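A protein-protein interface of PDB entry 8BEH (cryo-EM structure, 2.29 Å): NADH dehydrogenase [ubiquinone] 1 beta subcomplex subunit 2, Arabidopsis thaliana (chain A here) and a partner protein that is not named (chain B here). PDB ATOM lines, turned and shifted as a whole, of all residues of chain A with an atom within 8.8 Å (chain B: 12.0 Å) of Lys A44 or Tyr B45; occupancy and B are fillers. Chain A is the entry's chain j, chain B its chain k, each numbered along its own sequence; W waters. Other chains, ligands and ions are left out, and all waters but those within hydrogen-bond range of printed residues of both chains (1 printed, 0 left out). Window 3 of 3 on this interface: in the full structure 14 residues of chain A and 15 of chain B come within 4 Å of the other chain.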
ATOM      1  N   PHE A  37      23.143   0.489 -18.512  1.00  0.00           N
ATOM      2  CA  PHE A  37      22.885   0.672 -19.936  1.00  0.00           C
ATOM      3  C   PHE A  37      21.534   0.095 -20.327  1.00  0.00           C
ATOM      4  O   PHE A  37      20.798   0.697 -21.116  1.00  0.00           O
ATOM      5  CB  PHE A  37      23.992   0.025 -20.768  1.00  0.00           C
ATOM      6  CG  PHE A  37      23.767   0.120 -22.254  1.00  0.00           C
ATOM      7  CD1 PHE A  37      23.111  -0.889 -22.940  1.00  0.00           C
ATOM      8  CD2 PHE A  37      24.213   1.224 -22.965  1.00  0.00           C
ATOM      9  CE1 PHE A  37      22.902  -0.801 -24.298  1.00  0.00           C
ATOM     10  CE2 PHE A  37      24.008   1.315 -24.323  1.00  0.00           C
ATOM     11  CZ  PHE A  37      23.352   0.301 -24.992  1.00  0.00           C
ATOM     12  N   TRP A  38      21.198  -1.082 -19.797  1.00  0.00           N
ATOM     13  CA  TRP A  38      19.914  -1.698 -20.100  1.00  0.00           C
ATOM     14  C   TRP A  38      18.765  -0.826 -19.619  1.00  0.00           C
ATOM     15  O   TRP A  38      17.763  -0.662 -20.323  1.00  0.00           O
ATOM     16  CB  TRP A  38      19.860  -3.087 -19.467  1.00  0.00           C
ATOM     17  CG  TRP A  38      18.517  -3.727 -19.453  1.00  0.00           C
ATOM     18  CD1 TRP A  38      17.677  -3.831 -18.391  1.00  0.00           C
ATOM     19  CD2 TRP A  38      17.862  -4.370 -20.549  1.00  0.00           C
ATOM     20  NE1 TRP A  38      16.535  -4.501 -18.752  1.00  0.00           N
ATOM     21  CE2 TRP A  38      16.623  -4.840 -20.075  1.00  0.00           C
ATOM     22  CE3 TRP A  38      18.198  -4.584 -21.887  1.00  0.00           C
ATOM     23  CZ2 TRP A  38      15.723  -5.517 -20.892  1.00  0.00           C
ATOM     24  CZ3 TRP A  38      17.302  -5.260 -22.693  1.00  0.00           C
ATOM     25  CH2 TRP A  38      16.080  -5.715 -22.194  1.00  0.00           C
ATOM     26  N   ILE A  39      18.901  -0.244 -18.428  1.00  0.00           N
ATOM     27  CA  ILE A  39      17.861   0.644 -17.920  1.00  0.00           C
ATOM     28  C   ILE A  39      17.709   1.863 -18.822  1.00  0.00           C
ATOM     29  O   ILE A  39      16.592   2.271 -19.151  1.00  0.00           O
ATOM     30  CB  ILE A  39      18.162   1.044 -16.465  1.00  0.00           C
ATOM     31  CG1 ILE A  39      17.960  -0.154 -15.534  1.00  0.00           C
ATOM     32  CG2 ILE A  39      17.283   2.215 -16.031  1.00  0.00           C
ATOM     33  CD1 ILE A  39      18.505   0.060 -14.148  1.00  0.00           C
ATOM     34  N   LEU A  40      18.829   2.462 -19.240  1.00  0.00           N
ATOM     35  CA  LEU A  40      18.753   3.645 -20.098  1.00  0.00           C
ATOM     36  C   LEU A  40      18.113   3.319 -21.444  1.00  0.00           C
ATOM     37  O   LEU A  40      17.243   4.056 -21.927  1.00  0.00           O
ATOM     38  CB  LEU A  40      20.147   4.233 -20.295  1.00  0.00           C
ATOM     39  CG  LEU A  40      20.758   4.887 -19.058  1.00  0.00           C
ATOM     40  CD1 LEU A  40      22.165   5.370 -19.346  1.00  0.00           C
ATOM     41  CD2 LEU A  40      19.884   6.025 -18.553  1.00  0.00           C
ATOM     42  N   TYR A  41      18.526   2.208 -22.054  1.00  0.00           N
ATOM     43  CA  TYR A  41      17.986   1.803 -23.345  1.00  0.00           C
ATOM     44  C   TYR A  41      16.494   1.514 -23.248  1.00  0.00           C
ATOM     45  O   TYR A  41      15.705   1.969 -24.087  1.00  0.00           O
ATOM     46  CB  TYR A  41      18.756   0.584 -23.853  1.00  0.00           C
ATOM     47  CG  TYR A  41      18.336   0.068 -25.210  1.00  0.00           C
ATOM     48  CD1 TYR A  41      17.274  -0.818 -25.339  1.00  0.00           C
ATOM     49  CD2 TYR A  41      19.010   0.456 -26.361  1.00  0.00           C
ATOM     50  CE1 TYR A  41      16.893  -1.299 -26.566  1.00  0.00           C
ATOM     51  CE2 TYR A  41      18.630  -0.018 -27.595  1.00  0.00           C
ATOM     52  CZ  TYR A  41      17.571  -0.897 -27.691  1.00  0.00           C
ATOM     53  OH  TYR A  41      17.183  -1.374 -28.917  1.00  0.00           O
ATOM     54  N   ARG A  42      16.084   0.771 -22.213  1.00  0.00           N
ATOM     55  CA  ARG A  42      14.671   0.462 -22.037  1.00  0.00           C
ATOM     56  C   ARG A  42      13.864   1.722 -21.778  1.00  0.00           C
ATOM     57  O   ARG A  42      12.738   1.856 -22.269  1.00  0.00           O
ATOM     58  CB  ARG A  42      14.487  -0.529 -20.890  1.00  0.00           C
ATOM     59  CG  ARG A  42      14.766  -1.969 -21.254  1.00  0.00           C
ATOM     60  CD  ARG A  42      13.487  -2.729 -21.529  1.00  0.00           C
ATOM     61  NE  ARG A  42      12.910  -2.389 -22.825  1.00  0.00           N
ATOM     62  CZ  ARG A  42      13.411  -2.763 -23.994  1.00  0.00           C
ATOM     63  NH1 ARG A  42      14.520  -3.477 -24.074  1.00  0.00           N
ATOM     64  NH2 ARG A  42      12.781  -2.414 -25.110  1.00  0.00           N
ATOM     65  N   ALA A  43      14.411   2.648 -20.989  1.00  0.00           N
ATOM     66  CA  ALA A  43      13.714   3.899 -20.733  1.00  0.00           C
ATOM     67  C   ALA A  43      13.486   4.656 -22.031  1.00  0.00           C
ATOM     68  O   ALA A  43      12.362   5.057 -22.331  1.00  0.00           O
ATOM     69  CB  ALA A  43      14.497   4.744 -19.730  1.00  0.00           C
ATOM     70  N   LYS A  44      14.526   4.782 -22.854  1.00  0.00           N
ATOM     71  CA  LYS A  44      14.355   5.467 -24.130  1.00  0.00           C
ATOM     72  C   LYS A  44      13.335   4.757 -25.019  1.00  0.00           C
ATOM     73  O   LYS A  44      12.503   5.412 -25.657  1.00  0.00           O
ATOM     74  CB  LYS A  44      15.699   5.595 -24.841  1.00  0.00           C
ATOM     75  CG  LYS A  44      15.607   5.570 -26.345  1.00  0.00           C
ATOM     76  CD  LYS A  44      16.523   6.604 -26.959  1.00  0.00           C
ATOM     77  CE  LYS A  44      16.794   6.279 -28.409  1.00  0.00           C
ATOM     78  NZ  LYS A  44      17.395   4.924 -28.527  1.00  0.00           N
ATOM     79  N   GLN A  45      13.369   3.423 -25.065  1.00  0.00           N
ATOM     80  CA  GLN A  45      12.489   2.701 -25.981  1.00  0.00           C
ATOM     81  C   GLN A  45      11.030   2.776 -25.544  1.00  0.00           C
ATOM     82  O   GLN A  45      10.145   3.058 -26.359  1.00  0.00           O
ATOM     83  CB  GLN A  45      12.923   1.243 -26.114  1.00  0.00           C
ATOM     84  CG  GLN A  45      14.094   1.026 -27.046  1.00  0.00           C
ATOM     85  CD  GLN A  45      13.686   1.066 -28.501  1.00  0.00           C
ATOM     86  OE1 GLN A  45      14.154   1.912 -29.263  1.00  0.00           O
ATOM     87  NE2 GLN A  45      12.803   0.156 -28.896  1.00  0.00           N
ATOM     88  N   ASP A  46      10.750   2.522 -24.268  1.00  0.00           N
ATOM     89  CA  ASP A  46       9.365   2.402 -23.829  1.00  0.00           C
ATOM     90  C   ASP A  46       9.127   3.142 -22.520  1.00  0.00           C
ATOM     91  O   ASP A  46       8.492   2.620 -21.601  1.00  0.00           O
ATOM     92  CB  ASP A  46       8.955   0.934 -23.704  1.00  0.00           C
ATOM     93  CG  ASP A  46       9.978   0.101 -22.976  1.00  0.00           C
ATOM     94  OD1 ASP A  46      10.226   0.373 -21.785  1.00  0.00           O
ATOM     95  OD2 ASP A  46      10.542  -0.825 -23.595  1.00  0.00           O
ATOM     96  N   GLY A  47       9.610   4.375 -22.421  1.00  0.00           N
ATOM     97  CA  GLY A  47       9.321   5.216 -21.289  1.00  0.00           C
ATOM     98  C   GLY A  47       8.218   6.228 -21.524  1.00  0.00           C
ATOM     99  O   GLY A  47       7.457   6.548 -20.609  1.00  0.00           O
ATOM    100  N   PRO A  48       8.123   6.750 -22.793  1.00  0.00           N
ATOM    101  CA  PRO A  48       7.008   7.607 -23.122  1.00  0.00           C
ATOM    102  C   PRO A  48       5.750   6.753 -22.991  1.00  0.00           C
ATOM    103  O   PRO A  48       4.761   7.303 -22.627  1.00  0.00           O
ATOM    104  CB  PRO A  48       7.329   8.126 -24.514  1.00  0.00           C
ATOM    105  CG  PRO A  48       8.813   8.052 -24.584  1.00  0.00           C
ATOM    106  CD  PRO A  48       9.072   6.724 -23.932  1.00  0.00           C
ATOM    107  N   VAL A  49       5.825   5.449 -23.239  1.00  0.00           N
ATOM    108  CA  VAL A  49       4.532   4.691 -23.133  1.00  0.00           C
ATOM    109  C   VAL A  49       4.068   4.591 -21.674  1.00  0.00           C
ATOM    110  O   VAL A  49       2.913   4.879 -21.436  1.00  0.00           O
ATOM    111  CB  VAL A  49       4.543   3.363 -23.899  1.00  0.00           C
ATOM    112  CG1 VAL A  49       3.415   2.438 -23.481  1.00  0.00           C
ATOM    113  CG2 VAL A  49       4.540   3.576 -25.399  1.00  0.00           C
ATOM    114  N   TRP A  53       2.600   9.659 -22.377  1.00  0.00           N
ATOM    115  CA  TRP A  53       2.666  10.617 -23.508  1.00  0.00           C
ATOM    116  C   TRP A  53       2.029   9.969 -24.732  1.00  0.00           C
ATOM    117  O   TRP A  53       1.059  10.533 -25.240  1.00  0.00           O
ATOM    118  CB  TRP A  53       4.102  11.072 -23.746  1.00  0.00           C
ATOM    119  CG  TRP A  53       4.728  11.613 -22.504  1.00  0.00           C
ATOM    120  CD1 TRP A  53       4.087  12.235 -21.475  1.00  0.00           C
ATOM    121  CD2 TRP A  53       6.121  11.578 -22.155  1.00  0.00           C
ATOM    122  NE1 TRP A  53       4.988  12.605 -20.521  1.00  0.00           N
ATOM    123  CE2 TRP A  53       6.240  12.208 -20.902  1.00  0.00           C
ATOM    124  CE3 TRP A  53       7.272  11.087 -22.777  1.00  0.00           C
ATOM    125  CZ2 TRP A  53       7.464  12.356 -20.262  1.00  0.00           C
ATOM    126  CZ3 TRP A  53       8.483  11.224 -22.141  1.00  0.00           C
ATOM    127  CH2 TRP A  53       8.573  11.855 -20.900  1.00  0.00           C
ATOM    128  N   ARG A  54       2.475   8.787 -25.122  1.00  0.00           N
ATOM    129  CA  ARG A  54       1.942   8.142 -26.334  1.00  0.00           C
ATOM    130  C   ARG A  54       1.485   6.686 -26.143  1.00  0.00           C
ATOM    131  O   ARG A  54       1.633   6.147 -25.073  1.00  0.00           O
ATOM    132  CB  ARG A  54       3.024   8.083 -27.397  1.00  0.00           C
ATOM    133  CG  ARG A  54       4.308   7.428 -26.911  1.00  0.00           C
ATOM    134  CD  ARG A  54       5.355   7.357 -27.989  1.00  0.00           C
ATOM    135  NE  ARG A  54       4.828   6.628 -29.122  1.00  0.00           N
ATOM    136  CZ  ARG A  54       4.942   5.319 -29.289  1.00  0.00           C
ATOM    137  NH1 ARG A  54       5.569   4.589 -28.385  1.00  0.00           N
ATOM    138  NH2 ARG A  54       4.414   4.742 -30.350  1.00  0.00           N
ATOM    139  N   GLY B  36      29.580   4.999 -14.610  1.00  0.00           N
ATOM    140  CA  GLY B  36      30.292   5.734 -15.636  1.00  0.00           C
ATOM    141  C   GLY B  36      30.367   5.005 -16.960  1.00  0.00           C
ATOM    142  O   GLY B  36      30.063   5.582 -18.009  1.00  0.00           O
ATOM    143  N   ILE B  37      30.777   3.735 -16.920  1.00  0.00           N
ATOM    144  CA  ILE B  37      30.906   2.946 -18.143  1.00  0.00           C
ATOM    145  C   ILE B  37      29.558   2.789 -18.825  1.00  0.00           C
ATOM    146  O   ILE B  37      29.454   2.887 -20.053  1.00  0.00           O
ATOM    147  CB  ILE B  37      31.533   1.574 -17.836  1.00  0.00           C
ATOM    148  CG1 ILE B  37      32.778   1.735 -16.967  1.00  0.00           C
ATOM    149  CG2 ILE B  37      31.858   0.846 -19.126  1.00  0.00           C
ATOM    150  CD1 ILE B  37      32.821   0.787 -15.802  1.00  0.00           C
ATOM    151  N   GLY B  38      28.507   2.531 -18.045  1.00  0.00           N
ATOM    152  CA  GLY B  38      27.186   2.368 -18.626  1.00  0.00           C
ATOM    153  C   GLY B  38      26.690   3.628 -19.308  1.00  0.00           C
ATOM    154  O   GLY B  38      26.149   3.579 -20.414  1.00  0.00           O
ATOM    155  N   VAL B  39      26.873   4.778 -18.657  1.00  0.00           N
ATOM    156  CA  VAL B  39      26.437   6.041 -19.243  1.00  0.00           C
ATOM    157  C   VAL B  39      27.253   6.372 -20.488  1.00  0.00           C
ATOM    158  O   VAL B  39      26.705   6.828 -21.498  1.00  0.00           O
ATOM    159  CB  VAL B  39      26.507   7.166 -18.195  1.00  0.00           C
ATOM    160  CG1 VAL B  39      26.377   8.525 -18.863  1.00  0.00           C
ATOM    161  CG2 VAL B  39      25.401   6.989 -17.174  1.00  0.00           C
ATOM    162  N   GLY B  40      28.567   6.136 -20.448  1.00  0.00           N
ATOM    163  CA  GLY B  40      29.385   6.373 -21.628  1.00  0.00           C
ATOM    164  C   GLY B  40      29.001   5.483 -22.794  1.00  0.00           C
ATOM    165  O   GLY B  40      28.948   5.933 -23.945  1.00  0.00           O
ATOM    166  N   ALA B  41      28.724   4.209 -22.514  1.00  0.00           N
ATOM    167  CA  ALA B  41      28.280   3.296 -23.560  1.00  0.00           C
ATOM    168  C   ALA B  41      26.932   3.724 -24.123  1.00  0.00           C
ATOM    169  O   ALA B  41      26.705   3.645 -25.336  1.00  0.00           O
ATOM    170  CB  ALA B  41      28.218   1.869 -23.017  1.00  0.00           C
ATOM    171  N   PHE B  42      26.025   4.187 -23.259  1.00  0.00           N
ATOM    172  CA  PHE B  42      24.747   4.699 -23.738  1.00  0.00           C
ATOM    173  C   PHE B  42      24.938   5.912 -24.637  1.00  0.00           C
ATOM    174  O   PHE B  42      24.250   6.054 -25.652  1.00  0.00           O
ATOM    175  CB  PHE B  42      23.837   5.053 -22.568  1.00  0.00           C
ATOM    176  CG  PHE B  42      22.422   5.337 -22.973  1.00  0.00           C
ATOM    177  CD1 PHE B  42      21.694   4.409 -23.696  1.00  0.00           C
ATOM    178  CD2 PHE B  42      21.828   6.544 -22.655  1.00  0.00           C
ATOM    179  CE1 PHE B  42      20.395   4.676 -24.077  1.00  0.00           C
ATOM    180  CE2 PHE B  42      20.532   6.813 -23.032  1.00  0.00           C
ATOM    181  CZ  PHE B  42      19.815   5.877 -23.744  1.00  0.00           C
ATOM    182  N   CYS B  43      25.853   6.806 -24.270  1.00  0.00           N
ATOM    183  CA  CYS B  43      26.110   7.981 -25.099  1.00  0.00           C
ATOM    184  C   CYS B  43      26.669   7.585 -26.461  1.00  0.00           C
ATOM    185  O   CYS B  43      26.258   8.129 -27.494  1.00  0.00           O
ATOM    186  CB  CYS B  43      27.063   8.925 -24.375  1.00  0.00           C
ATOM    187  SG  CYS B  43      26.330   9.723 -22.929  1.00  0.00           S
ATOM    188  N   VAL B  44      27.604   6.633 -26.484  1.00  0.00           N
ATOM    189  CA  VAL B  44      28.165   6.178 -27.753  1.00  0.00           C
ATOM    190  C   VAL B  44      27.084   5.539 -28.619  1.00  0.00           C
ATOM    191  O   VAL B  44      27.000   5.802 -29.826  1.00  0.00           O
ATOM    192  CB  VAL B  44      29.335   5.213 -27.500  1.00  0.00           C
ATOM    193  CG1 VAL B  44      29.762   4.548 -28.791  1.00  0.00           C
ATOM    194  CG2 VAL B  44      30.496   5.955 -26.867  1.00  0.00           C
ATOM    195  N   TYR B  45      26.234   4.702 -28.016  1.00  0.00           N
ATOM    196  CA  TYR B  45      25.117   4.113 -28.749  1.00  0.00           C
ATOM    197  C   TYR B  45      24.180   5.181 -29.297  1.00  0.00           C
ATOM    198  O   TYR B  45      23.698   5.073 -30.428  1.00  0.00           O
ATOM    199  CB  TYR B  45      24.344   3.155 -27.842  1.00  0.00           C
ATOM    200  CG  TYR B  45      22.879   3.053 -28.197  1.00  0.00           C
ATOM    201  CD1 TYR B  45      22.447   2.240 -29.232  1.00  0.00           C
ATOM    202  CD2 TYR B  45      21.927   3.788 -27.501  1.00  0.00           C
ATOM    203  CE1 TYR B  45      21.110   2.152 -29.557  1.00  0.00           C
ATOM    204  CE2 TYR B  45      20.591   3.710 -27.823  1.00  0.00           C
ATOM    205  CZ  TYR B  45      20.189   2.892 -28.850  1.00  0.00           C
ATOM    206  OH  TYR B  45      18.855   2.812 -29.168  1.00  0.00           O
ATOM    207  N   LEU B  46      23.879   6.200 -28.491  1.00  0.00           N
ATOM    208  CA  LEU B  46      22.977   7.260 -28.927  1.00  0.00           C
ATOM    209  C   LEU B  46      23.554   8.010 -30.119  1.00  0.00           C
ATOM    210  O   LEU B  46      22.839   8.304 -31.084  1.00  0.00           O
ATOM    211  CB  LEU B  46      22.715   8.214 -27.764  1.00  0.00           C
ATOM    212  CG  LEU B  46      21.299   8.396 -27.217  1.00  0.00           C
ATOM    213  CD1 LEU B  46      21.320   9.418 -26.103  1.00  0.00           C
ATOM    214  CD2 LEU B  46      20.331   8.827 -28.309  1.00  0.00           C
ATOM    215  N   VAL B  47      24.850   8.324 -30.069  1.00  0.00           N
ATOM    216  CA  VAL B  47      25.490   8.990 -31.200  1.00  0.00           C
ATOM    217  C   VAL B  47      25.450   8.096 -32.431  1.00  0.00           C
ATOM    218  O   VAL B  47      25.156   8.556 -33.542  1.00  0.00           O
ATOM    219  CB  VAL B  47      26.927   9.408 -30.844  1.00  0.00           C
ATOM    220  CG1 VAL B  47      27.604  10.047 -32.039  1.00  0.00           C
ATOM    221  CG2 VAL B  47      26.910  10.384 -29.678  1.00  0.00           C
ATOM    222  N   GLY B  48      25.723   6.804 -32.253  1.00  0.00           N
ATOM    223  CA  GLY B  48      25.634   5.883 -33.371  1.00  0.00           C
ATOM    224  C   GLY B  48      24.244   5.811 -33.971  1.00  0.00           C
ATOM    225  O   GLY B  48      24.095   5.655 -35.185  1.00  0.00           O
ATOM    226  N   GLU B  49      23.211   5.926 -33.137  1.00  0.00           N
ATOM    227  CA  GLU B  49      21.844   5.869 -33.638  1.00  0.00           C
ATOM    228  C   GLU B  49      21.503   7.094 -34.476  1.00  0.00           C
ATOM    229  O   GLU B  49      20.576   7.046 -35.293  1.00  0.00           O
ATOM    230  CB  GLU B  49      20.868   5.720 -32.471  1.00  0.00           C
ATOM    231  CG  GLU B  49      19.434   5.382 -32.871  1.00  0.00           C
ATOM    232  CD  GLU B  49      19.228   3.912 -33.196  1.00  0.00           C
ATOM    233  OE1 GLU B  49      20.190   3.245 -33.634  1.00  0.00           O
ATOM    234  OE2 GLU B  49      18.094   3.420 -33.014  1.00  0.00           O
ATOM    235  N   GLN B  50      22.239   8.191 -34.295  1.00  0.00           N
ATOM    236  CA  GLN B  50      21.980   9.392 -35.078  1.00  0.00           C
ATOM    237  C   GLN B  50      22.259   9.156 -36.558  1.00  0.00           C
ATOM    238  O   GLN B  50      21.517   9.642 -37.419  1.00  0.00           O
ATOM    239  CB  GLN B  50      22.809  10.559 -34.537  1.00  0.00           C
ATOM    240  CG  GLN B  50      22.417  11.033 -33.146  1.00  0.00           C
ATOM    241  CD  GLN B  50      23.316  12.141 -32.631  1.00  0.00           C
ATOM    242  OE1 GLN B  50      24.467  12.265 -33.049  1.00  0.00           O
ATOM    243  NE2 GLN B  50      22.795  12.948 -31.714  1.00  0.00           N
ATOM    244  N   ILE B  51      23.313   8.410 -36.874  1.00  0.00           N
ATOM    245  CA  ILE B  51      23.597   8.093 -38.267  1.00  0.00           C
ATOM    246  C   ILE B  51      22.709   6.940 -38.735  1.00  0.00           C
ATOM    247  O   ILE B  51      21.511   6.906 -38.450  1.00  0.00           O
ATOM    248  CB  ILE B  51      25.119   7.812 -38.484  1.00  0.00           C
ATOM    249  CG1 ILE B  51      25.642   6.597 -37.693  1.00  0.00           C
ATOM    250  CG2 ILE B  51      25.939   9.048 -38.140  1.00  0.00           C
ATOM    251  CD1 ILE B  51      25.259   5.213 -38.217  1.00  0.00           C
HETATM  252  O   HOH W   1      16.801   2.536 -26.731  1.00  0.00           O
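Of the printed residues of chain B, Phe A37 touches Gly B38 (3.98 Å), Ala B41 (3.7 Å), Phe B42 (3.5 Å) and Tyr B45 (3.99 Å). Tyr A41 touches just these residues of chain B: Phe B42 and Tyr B45. Arg A42 touches none of the printed residues of chain B. No residue of chain B comes within 4 Å of Ala A43. Lys A44 touches just one residue of chain B: Tyr B45. Gly A47 touches none of the printed residues of chain B. Trp A53 touches none of the printed residues of chain B. Printed residues of chain A within 4 Å of Gly B38: Phe A37 (3.98 Å). Printed residues of chain A within 4 Å of Phe B42: Phe A37, Leu A40 and Tyr A41. Val B44 touches none of the printed residues of chain A. Printed residues of chain A within 4 Å of Tyr B45: Phe A37 (3.99 Å), Tyr A41 (3.2 Å) and Lys A44 (2.6 Å). The nearest residue of chain B that does not touch Lys A44 is Phe B42 (4.3 Å).
Among the printed residues, merely in contact across the chains: Tyr A41 with Tyr B45, Phe A37 with Phe B42, Leu A40 with Phe B42, Tyr A41 with Phe B42, Phe A37 with Ala B41, Phe A37 with Gly B38 and Phe A37 with Tyr B45.
Water W1 lies within hydrogen-bond range of O of Tyr A41 (2.9 Å), NZ of Lys A44 (3.0 Å) and OH of Tyr B45 (3.2 Å).
The side-chain hydroxyl of Tyr B45 is in hydrogen-bond range of the side-chain amino group of Lys A44, at 2.6 Å.
Hydrophobic or aromatic side chains of chain B that line the printed part of chain A: Phe B42 and Tyr B45. Among the printed residues, 8 pairs touch across the chains. Among the printed residues, no Asp or Glu carboxylate lies within 4 Å of a Lys or Arg side-chain nitrogen of the other chain.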
